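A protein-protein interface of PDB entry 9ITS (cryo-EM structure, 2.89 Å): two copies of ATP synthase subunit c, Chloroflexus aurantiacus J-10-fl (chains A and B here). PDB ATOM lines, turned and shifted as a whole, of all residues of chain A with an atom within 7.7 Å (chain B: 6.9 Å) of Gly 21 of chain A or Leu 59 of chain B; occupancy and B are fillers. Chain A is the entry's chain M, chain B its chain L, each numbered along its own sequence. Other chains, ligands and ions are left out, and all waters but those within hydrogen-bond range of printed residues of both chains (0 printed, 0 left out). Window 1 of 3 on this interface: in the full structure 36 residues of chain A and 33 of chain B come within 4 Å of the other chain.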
ATOM      1  N   VAL A  13      -7.631  10.366 -10.596  1.00  0.00           N
ATOM      2  CA  VAL A  13      -6.231  10.324 -10.191  1.00  0.00           C
ATOM      3  C   VAL A  13      -6.097  10.579  -8.695  1.00  0.00           C
ATOM      4  O   VAL A  13      -5.268   9.957  -8.021  1.00  0.00           O
ATOM      5  CB  VAL A  13      -5.400  11.318 -11.021  1.00  0.00           C
ATOM      6  CG1 VAL A  13      -3.948  11.276 -10.598  1.00  0.00           C
ATOM      7  CG2 VAL A  13      -5.512  10.984 -12.493  1.00  0.00           C
ATOM      8  N   GLY A  14      -6.923  11.469  -8.141  1.00  0.00           N
ATOM      9  CA  GLY A  14      -6.860  11.731  -6.715  1.00  0.00           C
ATOM     10  C   GLY A  14      -7.251  10.531  -5.874  1.00  0.00           C
ATOM     11  O   GLY A  14      -6.580  10.210  -4.892  1.00  0.00           O
ATOM     12  N   LEU A  15      -8.339   9.849  -6.245  1.00  0.00           N
ATOM     13  CA  LEU A  15      -8.744   8.667  -5.487  1.00  0.00           C
ATOM     14  C   LEU A  15      -7.727   7.539  -5.631  1.00  0.00           C
ATOM     15  O   LEU A  15      -7.425   6.834  -4.652  1.00  0.00           O
ATOM     16  CB  LEU A  15     -10.133   8.212  -5.930  1.00  0.00           C
ATOM     17  CG  LEU A  15     -11.270   9.222  -5.742  1.00  0.00           C
ATOM     18  CD1 LEU A  15     -12.523   8.775  -6.478  1.00  0.00           C
ATOM     19  CD2 LEU A  15     -11.565   9.450  -4.269  1.00  0.00           C
ATOM     20  N   GLY A  16      -7.187   7.350  -6.840  1.00  0.00           N
ATOM     21  CA  GLY A  16      -6.147   6.355  -7.034  1.00  0.00           C
ATOM     22  C   GLY A  16      -4.845   6.689  -6.340  1.00  0.00           C
ATOM     23  O   GLY A  16      -4.039   5.788  -6.089  1.00  0.00           O
ATOM     24  N   ALA A  17      -4.604   7.967  -6.055  1.00  0.00           N
ATOM     25  CA  ALA A  17      -3.470   8.335  -5.217  1.00  0.00           C
ATOM     26  C   ALA A  17      -3.771   8.101  -3.743  1.00  0.00           C
ATOM     27  O   ALA A  17      -2.883   7.698  -2.982  1.00  0.00           O
ATOM     28  CB  ALA A  17      -3.087   9.795  -5.461  1.00  0.00           C
ATOM     29  N   ILE A  18      -5.013   8.355  -3.321  1.00  0.00           N
ATOM     30  CA  ILE A  18      -5.351   8.248  -1.905  1.00  0.00           C
ATOM     31  C   ILE A  18      -5.308   6.796  -1.449  1.00  0.00           C
ATOM     32  O   ILE A  18      -4.690   6.468  -0.429  1.00  0.00           O
ATOM     33  CB  ILE A  18      -6.722   8.882  -1.617  1.00  0.00           C
ATOM     34  CG1 ILE A  18      -6.652  10.399  -1.744  1.00  0.00           C
ATOM     35  CG2 ILE A  18      -7.165   8.545  -0.206  1.00  0.00           C
ATOM     36  CD1 ILE A  18      -8.008  11.059  -1.834  1.00  0.00           C
ATOM     37  N   GLY A  19      -5.950   5.903  -2.198  1.00  0.00           N
ATOM     38  CA  GLY A  19      -6.083   4.531  -1.758  1.00  0.00           C
ATOM     39  C   GLY A  19      -4.784   3.746  -1.767  1.00  0.00           C
ATOM     40  O   GLY A  19      -4.253   3.339  -0.721  1.00  0.00           O
ATOM     41  N   PRO A  20      -4.259   3.499  -2.968  1.00  0.00           N
ATOM     42  CA  PRO A  20      -2.977   2.792  -3.081  1.00  0.00           C
ATOM     43  C   PRO A  20      -1.819   3.472  -2.373  1.00  0.00           C
ATOM     44  O   PRO A  20      -0.869   2.780  -2.004  1.00  0.00           O
ATOM     45  CB  PRO A  20      -2.753   2.739  -4.595  1.00  0.00           C
ATOM     46  CG  PRO A  20      -4.132   2.644  -5.147  1.00  0.00           C
ATOM     47  CD  PRO A  20      -5.013   3.467  -4.232  1.00  0.00           C
ATOM     48  N   GLY A  21      -1.857   4.790  -2.166  1.00  0.00           N
ATOM     49  CA  GLY A  21      -0.801   5.425  -1.390  1.00  0.00           C
ATOM     50  C   GLY A  21      -0.772   4.944   0.049  1.00  0.00           C
ATOM     51  O   GLY A  21       0.284   4.584   0.582  1.00  0.00           O
ATOM     52  N   VAL A  22      -1.942   4.905   0.690  1.00  0.00           N
ATOM     53  CA  VAL A  22      -2.031   4.386   2.051  1.00  0.00           C
ATOM     54  C   VAL A  22      -1.715   2.897   2.073  1.00  0.00           C
ATOM     55  O   VAL A  22      -1.080   2.398   3.011  1.00  0.00           O
ATOM     56  CB  VAL A  22      -3.419   4.689   2.645  1.00  0.00           C
ATOM     57  CG1 VAL A  22      -3.533   4.135   4.056  1.00  0.00           C
ATOM     58  CG2 VAL A  22      -3.672   6.187   2.648  1.00  0.00           C
ATOM     59  N   GLY A  23      -2.143   2.165   1.038  1.00  0.00           N
ATOM     60  CA  GLY A  23      -1.790   0.753   0.959  1.00  0.00           C
ATOM     61  C   GLY A  23      -0.290   0.525   0.884  1.00  0.00           C
ATOM     62  O   GLY A  23       0.251  -0.347   1.571  1.00  0.00           O
ATOM     63  N   ILE A  24       0.400   1.319   0.061  1.00  0.00           N
ATOM     64  CA  ILE A  24       1.852   1.228  -0.062  1.00  0.00           C
ATOM     65  C   ILE A  24       2.518   1.564   1.264  1.00  0.00           C
ATOM     66  O   ILE A  24       3.461   0.884   1.694  1.00  0.00           O
ATOM     67  CB  ILE A  24       2.341   2.154  -1.194  1.00  0.00           C
ATOM     68  CG1 ILE A  24       2.099   1.511  -2.559  1.00  0.00           C
ATOM     69  CG2 ILE A  24       3.811   2.513  -1.019  1.00  0.00           C
ATOM     70  CD1 ILE A  24       2.153   2.487  -3.713  1.00  0.00           C
ATOM     71  N   GLY A  25       2.042   2.621   1.926  1.00  0.00           N
ATOM     72  CA  GLY A  25       2.603   2.984   3.219  1.00  0.00           C
ATOM     73  C   GLY A  25       2.469   1.873   4.240  1.00  0.00           C
ATOM     74  O   GLY A  25       3.432   1.525   4.932  1.00  0.00           O
ATOM     75  N   ILE A  26       1.275   1.280   4.325  1.00  0.00           N
ATOM     76  CA  ILE A  26       1.033   0.198   5.276  1.00  0.00           C
ATOM     77  C   ILE A  26       1.914  -1.004   4.956  1.00  0.00           C
ATOM     78  O   ILE A  26       2.517  -1.607   5.856  1.00  0.00           O
ATOM     79  CB  ILE A  26      -0.462  -0.171   5.279  1.00  0.00           C
ATOM     80  CG1 ILE A  26      -1.270   0.895   6.020  1.00  0.00           C
ATOM     81  CG2 ILE A  26      -0.687  -1.531   5.908  1.00  0.00           C
ATOM     82  CD1 ILE A  26      -2.759   0.804   5.781  1.00  0.00           C
ATOM     83  N   ILE A  27       2.020  -1.356   3.672  1.00  0.00           N
ATOM     84  CA  ILE A  27       2.811  -2.519   3.270  1.00  0.00           C
ATOM     85  C   ILE A  27       4.274  -2.324   3.636  1.00  0.00           C
ATOM     86  O   ILE A  27       4.906  -3.201   4.241  1.00  0.00           O
ATOM     87  CB  ILE A  27       2.645  -2.778   1.763  1.00  0.00           C
ATOM     88  CG1 ILE A  27       1.289  -3.412   1.489  1.00  0.00           C
ATOM     89  CG2 ILE A  27       3.763  -3.671   1.246  1.00  0.00           C
ATOM     90  CD1 ILE A  27       0.922  -3.452   0.037  1.00  0.00           C
ATOM     91  N   ILE A  53       2.929  -4.293  -3.086  1.00  0.00           N
ATOM     92  CA  ILE A  53       3.154  -2.988  -3.703  1.00  0.00           C
ATOM     93  C   ILE A  53       2.714  -3.016  -5.161  1.00  0.00           C
ATOM     94  O   ILE A  53       2.155  -2.041  -5.678  1.00  0.00           O
ATOM     95  CB  ILE A  53       4.630  -2.575  -3.556  1.00  0.00           C
ATOM     96  CG1 ILE A  53       4.983  -2.371  -2.084  1.00  0.00           C
ATOM     97  CG2 ILE A  53       4.915  -1.303  -4.334  1.00  0.00           C
ATOM     98  CD1 ILE A  53       4.395  -1.126  -1.478  1.00  0.00           C
ATOM     99  N   THR A  56      -1.124  -2.751  -5.237  1.00  0.00           N
ATOM    100  CA  THR A  56      -1.541  -1.376  -4.960  1.00  0.00           C
ATOM    101  C   THR A  56      -1.280  -0.468  -6.159  1.00  0.00           C
ATOM    102  O   THR A  56      -2.152   0.310  -6.574  1.00  0.00           O
ATOM    103  CB  THR A  56      -0.815  -0.842  -3.726  1.00  0.00           C
ATOM    104  OG1 THR A  56       0.600  -0.938  -3.930  1.00  0.00           O
ATOM    105  CG2 THR A  56      -1.199  -1.632  -2.487  1.00  0.00           C
ATOM    106  N   GLU A  57      -0.079  -0.562  -6.736  1.00  0.00           N
ATOM    107  CA  GLU A  57       0.229   0.226  -7.922  1.00  0.00           C
ATOM    108  C   GLU A  57      -0.635  -0.188  -9.101  1.00  0.00           C
ATOM    109  O   GLU A  57      -0.915   0.634  -9.970  1.00  0.00           O
ATOM    110  CB  GLU A  57       1.709   0.100  -8.282  1.00  0.00           C
ATOM    111  CG  GLU A  57       2.190   1.181  -9.240  1.00  0.00           C
ATOM    112  CD  GLU A  57       3.699   1.253  -9.338  1.00  0.00           C
ATOM    113  OE1 GLU A  57       4.326   0.216  -9.638  1.00  0.00           O
ATOM    114  OE2 GLU A  57       4.258   2.350  -9.124  1.00  0.00           O
ATOM    115  N   ALA A  58      -1.072  -1.447  -9.146  1.00  0.00           N
ATOM    116  CA  ALA A  58      -1.983  -1.878 -10.199  1.00  0.00           C
ATOM    117  C   ALA A  58      -3.314  -1.153 -10.091  1.00  0.00           C
ATOM    118  O   ALA A  58      -3.865  -0.699 -11.095  1.00  0.00           O
ATOM    119  CB  ALA A  58      -2.185  -3.391 -10.136  1.00  0.00           C
ATOM    120  N   LEU A  59      -3.839  -1.023  -8.872  1.00  0.00           N
ATOM    121  CA  LEU A  59      -5.081  -0.266  -8.694  1.00  0.00           C
ATOM    122  C   LEU A  59      -4.888   1.210  -9.049  1.00  0.00           C
ATOM    123  O   LEU A  59      -5.720   1.818  -9.745  1.00  0.00           O
ATOM    124  CB  LEU A  59      -5.592  -0.421  -7.263  1.00  0.00           C
ATOM    125  CG  LEU A  59      -5.904  -1.855  -6.829  1.00  0.00           C
ATOM    126  CD1 LEU A  59      -6.509  -1.878  -5.435  1.00  0.00           C
ATOM    127  CD2 LEU A  59      -6.831  -2.530  -7.828  1.00  0.00           C
ATOM    128  N   ALA A  60      -3.778   1.799  -8.593  1.00  0.00           N
ATOM    129  CA  ALA A  60      -3.510   3.204  -8.894  1.00  0.00           C
ATOM    130  C   ALA A  60      -3.354   3.427 -10.396  1.00  0.00           C
ATOM    131  O   ALA A  60      -3.830   4.428 -10.946  1.00  0.00           O
ATOM    132  CB  ALA A  60      -2.262   3.673  -8.148  1.00  0.00           C
ATOM    133  N   ILE A  61      -2.690   2.494 -11.078  1.00  0.00           N
ATOM    134  CA  ILE A  61      -2.479   2.605 -12.513  1.00  0.00           C
ATOM    135  C   ILE A  61      -3.768   2.324 -13.274  1.00  0.00           C
ATOM    136  O   ILE A  61      -3.978   2.869 -14.358  1.00  0.00           O
ATOM    137  CB  ILE A  61      -1.315   1.681 -12.933  1.00  0.00           C
ATOM    138  CG1 ILE A  61       0.018   2.284 -12.483  1.00  0.00           C
ATOM    139  CG2 ILE A  61      -1.273   1.469 -14.423  1.00  0.00           C
ATOM    140  CD1 ILE A  61       0.282   3.665 -13.039  1.00  0.00           C
ATOM    141  N   LEU A  64      -5.196   5.708 -13.193  1.00  0.00           N
ATOM    142  CA  LEU A  64      -4.491   6.611 -14.100  1.00  0.00           C
ATOM    143  C   LEU A  64      -4.776   6.280 -15.564  1.00  0.00           C
ATOM    144  O   LEU A  64      -4.875   7.180 -16.404  1.00  0.00           O
ATOM    145  CB  LEU A  64      -2.991   6.559 -13.814  1.00  0.00           C
ATOM    146  CG  LEU A  64      -2.139   7.704 -14.359  1.00  0.00           C
ATOM    147  CD1 LEU A  64      -2.748   9.046 -13.996  1.00  0.00           C
ATOM    148  CD2 LEU A  64      -0.728   7.598 -13.813  1.00  0.00           C
ATOM    149  N   GLY B  16      -4.641  14.500  -4.746  1.00  0.00           N
ATOM    150  CA  GLY B  16      -3.439  13.732  -5.006  1.00  0.00           C
ATOM    151  C   GLY B  16      -2.401  13.767  -3.907  1.00  0.00           C
ATOM    152  O   GLY B  16      -1.416  13.028  -3.985  1.00  0.00           O
ATOM    153  N   GLY B  19      -3.468  10.707   0.209  1.00  0.00           N
ATOM    154  CA  GLY B  19      -2.960   9.368   0.386  1.00  0.00           C
ATOM    155  C   GLY B  19      -1.450   9.236   0.380  1.00  0.00           C
ATOM    156  O   GLY B  19      -0.884   8.509   1.202  1.00  0.00           O
ATOM    157  N   PRO B  20      -0.764   9.885  -0.572  1.00  0.00           N
ATOM    158  CA  PRO B  20       0.707   9.876  -0.516  1.00  0.00           C
ATOM    159  C   PRO B  20       1.277  10.424   0.779  1.00  0.00           C
ATOM    160  O   PRO B  20       2.273   9.889   1.271  1.00  0.00           O
ATOM    161  CB  PRO B  20       1.096  10.736  -1.724  1.00  0.00           C
ATOM    162  CG  PRO B  20       0.029  10.450  -2.703  1.00  0.00           C
ATOM    163  CD  PRO B  20      -1.241  10.324  -1.897  1.00  0.00           C
ATOM    164  N   GLY B  21       0.671  11.462   1.359  1.00  0.00           N
ATOM    165  CA  GLY B  21       1.176  11.982   2.622  1.00  0.00           C
ATOM    166  C   GLY B  21       1.044  10.985   3.758  1.00  0.00           C
ATOM    167  O   GLY B  21       1.980  10.780   4.538  1.00  0.00           O
ATOM    168  N   VAL B  22      -0.122  10.343   3.859  1.00  0.00           N
ATOM    169  CA  VAL B  22      -0.334   9.326   4.885  1.00  0.00           C
ATOM    170  C   VAL B  22       0.601   8.145   4.667  1.00  0.00           C
ATOM    171  O   VAL B  22       1.152   7.588   5.624  1.00  0.00           O
ATOM    172  CB  VAL B  22      -1.810   8.887   4.904  1.00  0.00           C
ATOM    173  CG1 VAL B  22      -2.058   7.899   6.031  1.00  0.00           C
ATOM    174  CG2 VAL B  22      -2.718  10.094   5.051  1.00  0.00           C
ATOM    175  N   GLY B  23       0.792   7.741   3.409  1.00  0.00           N
ATOM    176  CA  GLY B  23       1.711   6.655   3.119  1.00  0.00           C
ATOM    177  C   GLY B  23       3.144   6.989   3.488  1.00  0.00           C
ATOM    178  O   GLY B  23       3.859   6.152   4.041  1.00  0.00           O
ATOM    179  N   ILE B  24       3.578   8.219   3.198  1.00  0.00           N
ATOM    180  CA  ILE B  24       4.920   8.655   3.572  1.00  0.00           C
ATOM    181  C   ILE B  24       5.079   8.638   5.086  1.00  0.00           C
ATOM    182  O   ILE B  24       6.090   8.158   5.615  1.00  0.00           O
ATOM    183  CB  ILE B  24       5.207  10.053   2.992  1.00  0.00           C
ATOM    184  CG1 ILE B  24       5.401   9.983   1.476  1.00  0.00           C
ATOM    185  CG2 ILE B  24       6.423  10.679   3.661  1.00  0.00           C
ATOM    186  CD1 ILE B  24       5.202  11.307   0.773  1.00  0.00           C
ATOM    187  N   ILE B  26       3.361   6.868   7.345  1.00  0.00           N
ATOM    188  CA  ILE B  26       3.342   5.497   7.839  1.00  0.00           C
ATOM    189  C   ILE B  26       4.657   4.793   7.516  1.00  0.00           C
ATOM    190  O   ILE B  26       5.194   4.048   8.343  1.00  0.00           O
ATOM    191  CB  ILE B  26       2.126   4.749   7.261  1.00  0.00           C
ATOM    192  CG1 ILE B  26       0.836   5.270   7.895  1.00  0.00           C
ATOM    193  CG2 ILE B  26       2.234   3.259   7.497  1.00  0.00           C
ATOM    194  CD1 ILE B  26      -0.419   4.750   7.234  1.00  0.00           C
ATOM    195  N   ILE B  27       5.208   5.041   6.325  1.00  0.00           N
ATOM    196  CA  ILE B  27       6.471   4.421   5.932  1.00  0.00           C
ATOM    197  C   ILE B  27       7.599   4.887   6.842  1.00  0.00           C
ATOM    198  O   ILE B  27       8.412   4.085   7.315  1.00  0.00           O
ATOM    199  CB  ILE B  27       6.776   4.730   4.455  1.00  0.00           C
ATOM    200  CG1 ILE B  27       6.018   3.771   3.546  1.00  0.00           C
ATOM    201  CG2 ILE B  27       8.262   4.629   4.171  1.00  0.00           C
ATOM    202  CD1 ILE B  27       6.031   4.170   2.094  1.00  0.00           C
ATOM    203  N   ILE B  53       9.273   5.045  -0.467  1.00  0.00           N
ATOM    204  CA  ILE B  53       9.051   6.480  -0.587  1.00  0.00           C
ATOM    205  C   ILE B  53       8.872   6.835  -2.056  1.00  0.00           C
ATOM    206  O   ILE B  53       7.937   7.568  -2.417  1.00  0.00           O
ATOM    207  CB  ILE B  53      10.178   7.288   0.103  1.00  0.00           C
ATOM    208  CG1 ILE B  53       9.691   8.688   0.460  1.00  0.00           C
ATOM    209  CG2 ILE B  53      11.411   7.483  -0.754  1.00  0.00           C
ATOM    210  CD1 ILE B  53       8.690   8.693   1.568  1.00  0.00           C
ATOM    211  N   ALA B  54       9.653   6.190  -2.936  1.00  0.00           N
ATOM    212  CA  ALA B  54       9.537   6.470  -4.359  1.00  0.00           C
ATOM    213  C   ALA B  54       8.131   6.166  -4.836  1.00  0.00           C
ATOM    214  O   ALA B  54       7.482   7.018  -5.461  1.00  0.00           O
ATOM    215  CB  ALA B  54      10.567   5.662  -5.146  1.00  0.00           C
ATOM    216  N   PHE B  55       7.607   5.000  -4.443  1.00  0.00           N
ATOM    217  CA  PHE B  55       6.265   4.619  -4.858  1.00  0.00           C
ATOM    218  C   PHE B  55       5.261   5.673  -4.431  1.00  0.00           C
ATOM    219  O   PHE B  55       4.468   6.151  -5.255  1.00  0.00           O
ATOM    220  CB  PHE B  55       5.905   3.252  -4.281  1.00  0.00           C
ATOM    221  CG  PHE B  55       6.369   2.102  -5.124  1.00  0.00           C
ATOM    222  CD1 PHE B  55       5.694   1.758  -6.283  1.00  0.00           C
ATOM    223  CD2 PHE B  55       7.489   1.370  -4.766  1.00  0.00           C
ATOM    224  CE1 PHE B  55       6.122   0.702  -7.063  1.00  0.00           C
ATOM    225  CE2 PHE B  55       7.921   0.314  -5.543  1.00  0.00           C
ATOM    226  CZ  PHE B  55       7.235  -0.019  -6.692  1.00  0.00           C
ATOM    227  N   THR B  56       5.350   6.124  -3.174  1.00  0.00           N
ATOM    228  CA  THR B  56       4.420   7.144  -2.707  1.00  0.00           C
ATOM    229  C   THR B  56       4.560   8.398  -3.550  1.00  0.00           C
ATOM    230  O   THR B  56       3.572   8.893  -4.115  1.00  0.00           O
ATOM    231  CB  THR B  56       4.661   7.451  -1.230  1.00  0.00           C
ATOM    232  OG1 THR B  56       6.041   7.778  -1.025  1.00  0.00           O
ATOM    233  CG2 THR B  56       4.295   6.250  -0.374  1.00  0.00           C
ATOM    234  N   GLU B  57       5.804   8.851  -3.742  1.00  0.00           N
ATOM    235  CA  GLU B  57       6.034  10.043  -4.543  1.00  0.00           C
ATOM    236  C   GLU B  57       5.480   9.850  -5.941  1.00  0.00           C
ATOM    237  O   GLU B  57       4.835  10.755  -6.489  1.00  0.00           O
ATOM    238  CB  GLU B  57       7.527  10.372  -4.587  1.00  0.00           C
ATOM    239  CG  GLU B  57       8.092  10.831  -3.254  1.00  0.00           C
ATOM    240  CD  GLU B  57       7.489  12.140  -2.783  1.00  0.00           C
ATOM    241  OE1 GLU B  57       7.169  12.992  -3.638  1.00  0.00           O
ATOM    242  OE2 GLU B  57       7.334  12.317  -1.556  1.00  0.00           O
ATOM    243  N   ALA B  58       5.639   8.635  -6.485  1.00  0.00           N
ATOM    244  CA  ALA B  58       5.126   8.339  -7.815  1.00  0.00           C
ATOM    245  C   ALA B  58       3.654   8.692  -7.899  1.00  0.00           C
ATOM    246  O   ALA B  58       3.254   9.534  -8.715  1.00  0.00           O
ATOM    247  CB  ALA B  58       5.345   6.863  -8.145  1.00  0.00           C
ATOM    248  N   LEU B  59       2.857   8.162  -6.965  1.00  0.00           N
ATOM    249  CA  LEU B  59       1.429   8.442  -6.997  1.00  0.00           C
ATOM    250  C   LEU B  59       1.188   9.937  -6.907  1.00  0.00           C
ATOM    251  O   LEU B  59       0.493  10.513  -7.756  1.00  0.00           O
ATOM    252  CB  LEU B  59       0.716   7.701  -5.866  1.00  0.00           C
ATOM    253  CG  LEU B  59       0.772   6.171  -5.907  1.00  0.00           C
ATOM    254  CD1 LEU B  59      -0.358   5.577  -5.085  1.00  0.00           C
ATOM    255  CD2 LEU B  59       0.723   5.650  -7.337  1.00  0.00           C
ATOM    256  N   ALA B  60       1.867  10.596  -5.961  1.00  0.00           N
ATOM    257  CA  ALA B  60       1.706  12.034  -5.804  1.00  0.00           C
ATOM    258  C   ALA B  60       2.060  12.750  -7.095  1.00  0.00           C
ATOM    259  O   ALA B  60       1.265  13.546  -7.615  1.00  0.00           O
ATOM    260  CB  ALA B  60       2.567  12.537  -4.647  1.00  0.00           C
ATOM    261  N   ILE B  61       3.207  12.397  -7.684  1.00  0.00           N
ATOM    262  CA  ILE B  61       3.647  13.157  -8.843  1.00  0.00           C
ATOM    263  C   ILE B  61       2.705  12.903 -10.005  1.00  0.00           C
ATOM    264  O   ILE B  61       2.476  13.802 -10.829  1.00  0.00           O
ATOM    265  CB  ILE B  61       5.121  12.859  -9.192  1.00  0.00           C
ATOM    266  CG1 ILE B  61       5.702  14.016 -10.002  1.00  0.00           C
ATOM    267  CG2 ILE B  61       5.272  11.571  -9.983  1.00  0.00           C
ATOM    268  CD1 ILE B  61       5.781  15.310  -9.230  1.00  0.00           C
ATOM    269  N   PHE B  62       2.073  11.718 -10.040  1.00  0.00           N
ATOM    270  CA  PHE B  62       1.084  11.447 -11.075  1.00  0.00           C
ATOM    271  C   PHE B  62       0.008  12.517 -11.058  1.00  0.00           C
ATOM    272  O   PHE B  62      -0.239  13.182 -12.075  1.00  0.00           O
ATOM    273  CB  PHE B  62       0.469  10.059 -10.881  1.00  0.00           C
ATOM    274  CG  PHE B  62       1.436   8.926 -11.087  1.00  0.00           C
ATOM    275  CD1 PHE B  62       2.619   9.117 -11.783  1.00  0.00           C
ATOM    276  CD2 PHE B  62       1.157   7.665 -10.583  1.00  0.00           C
ATOM    277  CE1 PHE B  62       3.508   8.074 -11.967  1.00  0.00           C
ATOM    278  CE2 PHE B  62       2.041   6.618 -10.767  1.00  0.00           C
ATOM    279  CZ  PHE B  62       3.216   6.822 -11.460  1.00  0.00           C
ATOM    280  N   GLY B  63      -0.561  12.771  -9.874  1.00  0.00           N
ATOM    281  CA  GLY B  63      -1.556  13.820  -9.760  1.00  0.00           C
ATOM    282  C   GLY B  63      -1.019  15.153 -10.228  1.00  0.00           C
ATOM    283  O   GLY B  63      -1.655  15.838 -11.036  1.00  0.00           O
ATOM    284  N   LEU B  64       0.207  15.487  -9.808  1.00  0.00           N
ATOM    285  CA  LEU B  64       0.795  16.756 -10.209  1.00  0.00           C
ATOM    286  C   LEU B  64       0.905  16.832 -11.722  1.00  0.00           C
ATOM    287  O   LEU B  64       0.519  17.842 -12.327  1.00  0.00           O
ATOM    288  CB  LEU B  64       2.161  16.939  -9.550  1.00  0.00           C
ATOM    289  CG  LEU B  64       2.598  18.389  -9.338  1.00  0.00           C
ATOM    290  CD1 LEU B  64       1.529  19.159  -8.578  1.00  0.00           C
ATOM    291  CD2 LEU B  64       3.926  18.456  -8.604  1.00  0.00           C
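Among the printed residues, merely in contact across the chains: Glu 57 of chain A with Phe 55 of chain B, Ala 17 of chain A with Pro 20 of chain B, Gly 25 of chain A with Ile 26 of chain B, Gly 21 of chain A with Leu 59 of chain B, Ile 18 of chain A with Gly 19 of chain B, Gly 25 of chain A with Gly 23 of chain B, Gly 25 of chain A with Ile 27 of chain B, Ile 53 of chain A with Phe 55 of chain B, Gly 21 of chain A with Gly 23 of chain B, Val 13 of chain A with Gly 63 of chain B, Ala 60 of chain A with Leu 59 of chain B, Leu 64 of chain A with Phe 62 of chain B, Pro 20 of chain A with Leu 59 of chain B, Gly 21 of chain A with Gly 19 of chain B, Ala 17 of chain A with Gly 19 of chain B, Val 22 of chain A with Gly 19 of chain B, Gly 16 of chain A with Leu 59 of chain B, Ile 24 of chain A with Thr 56 of chain B, Ile 26 of chain A with Ile 26 of chain B, Ile 24 of chain A with Phe 55 of chain B, Ala 17 of chain A with Leu 59 of chain B, Ala 17 of chain A with Gly 16 of chain B and Val 22 of chain A with Val 22 of chain B.
O of Ile 53 of chain A lies within hydrogen-bond range of OG1 of Thr 56 of chain A.
Of the printed residues of chain B, Val 13 of chain A touches Gly 63. Printed residues of chain B within 4 Å of Gly 21 of chain A: Gly 19 (3.7 Å), Gly 23 (3.6 Å) and Leu 59 (3.4 Å). Of the printed residues of chain A, Gly 23 of chain B touches Gly 21 and Gly 25. No residue of chain A comes within 4 Å of Ala 58 of chain B. Of the printed residues of chain A, Leu 59 of chain B touches Gly 16 (3.8 Å), Ala 17 (3.9 Å), Pro 20 (3.7 Å), Gly 21 (3.4 Å) and Ala 60 (3.7 Å). The nearest printed residue of chain B that does not touch Gly 16 of chain A is Pro 20 of chain B (6.8 Å).
Pro 20 of chain A touches Leu 59 of chain B, but with the chains exchanged Leu 59 of chain A does not touch Pro 20 of chain B (12.1 Å). Gly 21 of chain A touches Gly 19 of chain B, but with the chains exchanged Gly 19 of chain A does not touch Gly 21 of chain B (9.3 Å). Gly 21 of chain A touches Leu 59 of chain B, but with the chains exchanged Leu 59 of chain A does not touch Gly 21 of chain B (15.6 Å). Val 22 of chain A touches Gly 19 of chain B, but with the chains exchanged Gly 19 of chain A does not touch Val 22 of chain B (8.3 Å).
Of the 23 printed residues of chain A, 14 touch a printed residue of chain B. Printed residues of chain A that touch a printed residue of chain B: Val 13, Gly 16, Ala 17, Ile 18, Pro 20, Gly 21, Val 22, Ile 24, Gly 25, Ile 26, Ile 53, Glu 57, Ala 60 and Leu 64. Of the 21 printed residues of chain B, 12 touch a printed residue of chain A. Among the printed residues, 23 pairs touch across the chains. Among the printed residues, no Asp or Glu carboxylate lies within 4 Å of a Lys or Arg side-chain nitrogen of the other chain.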
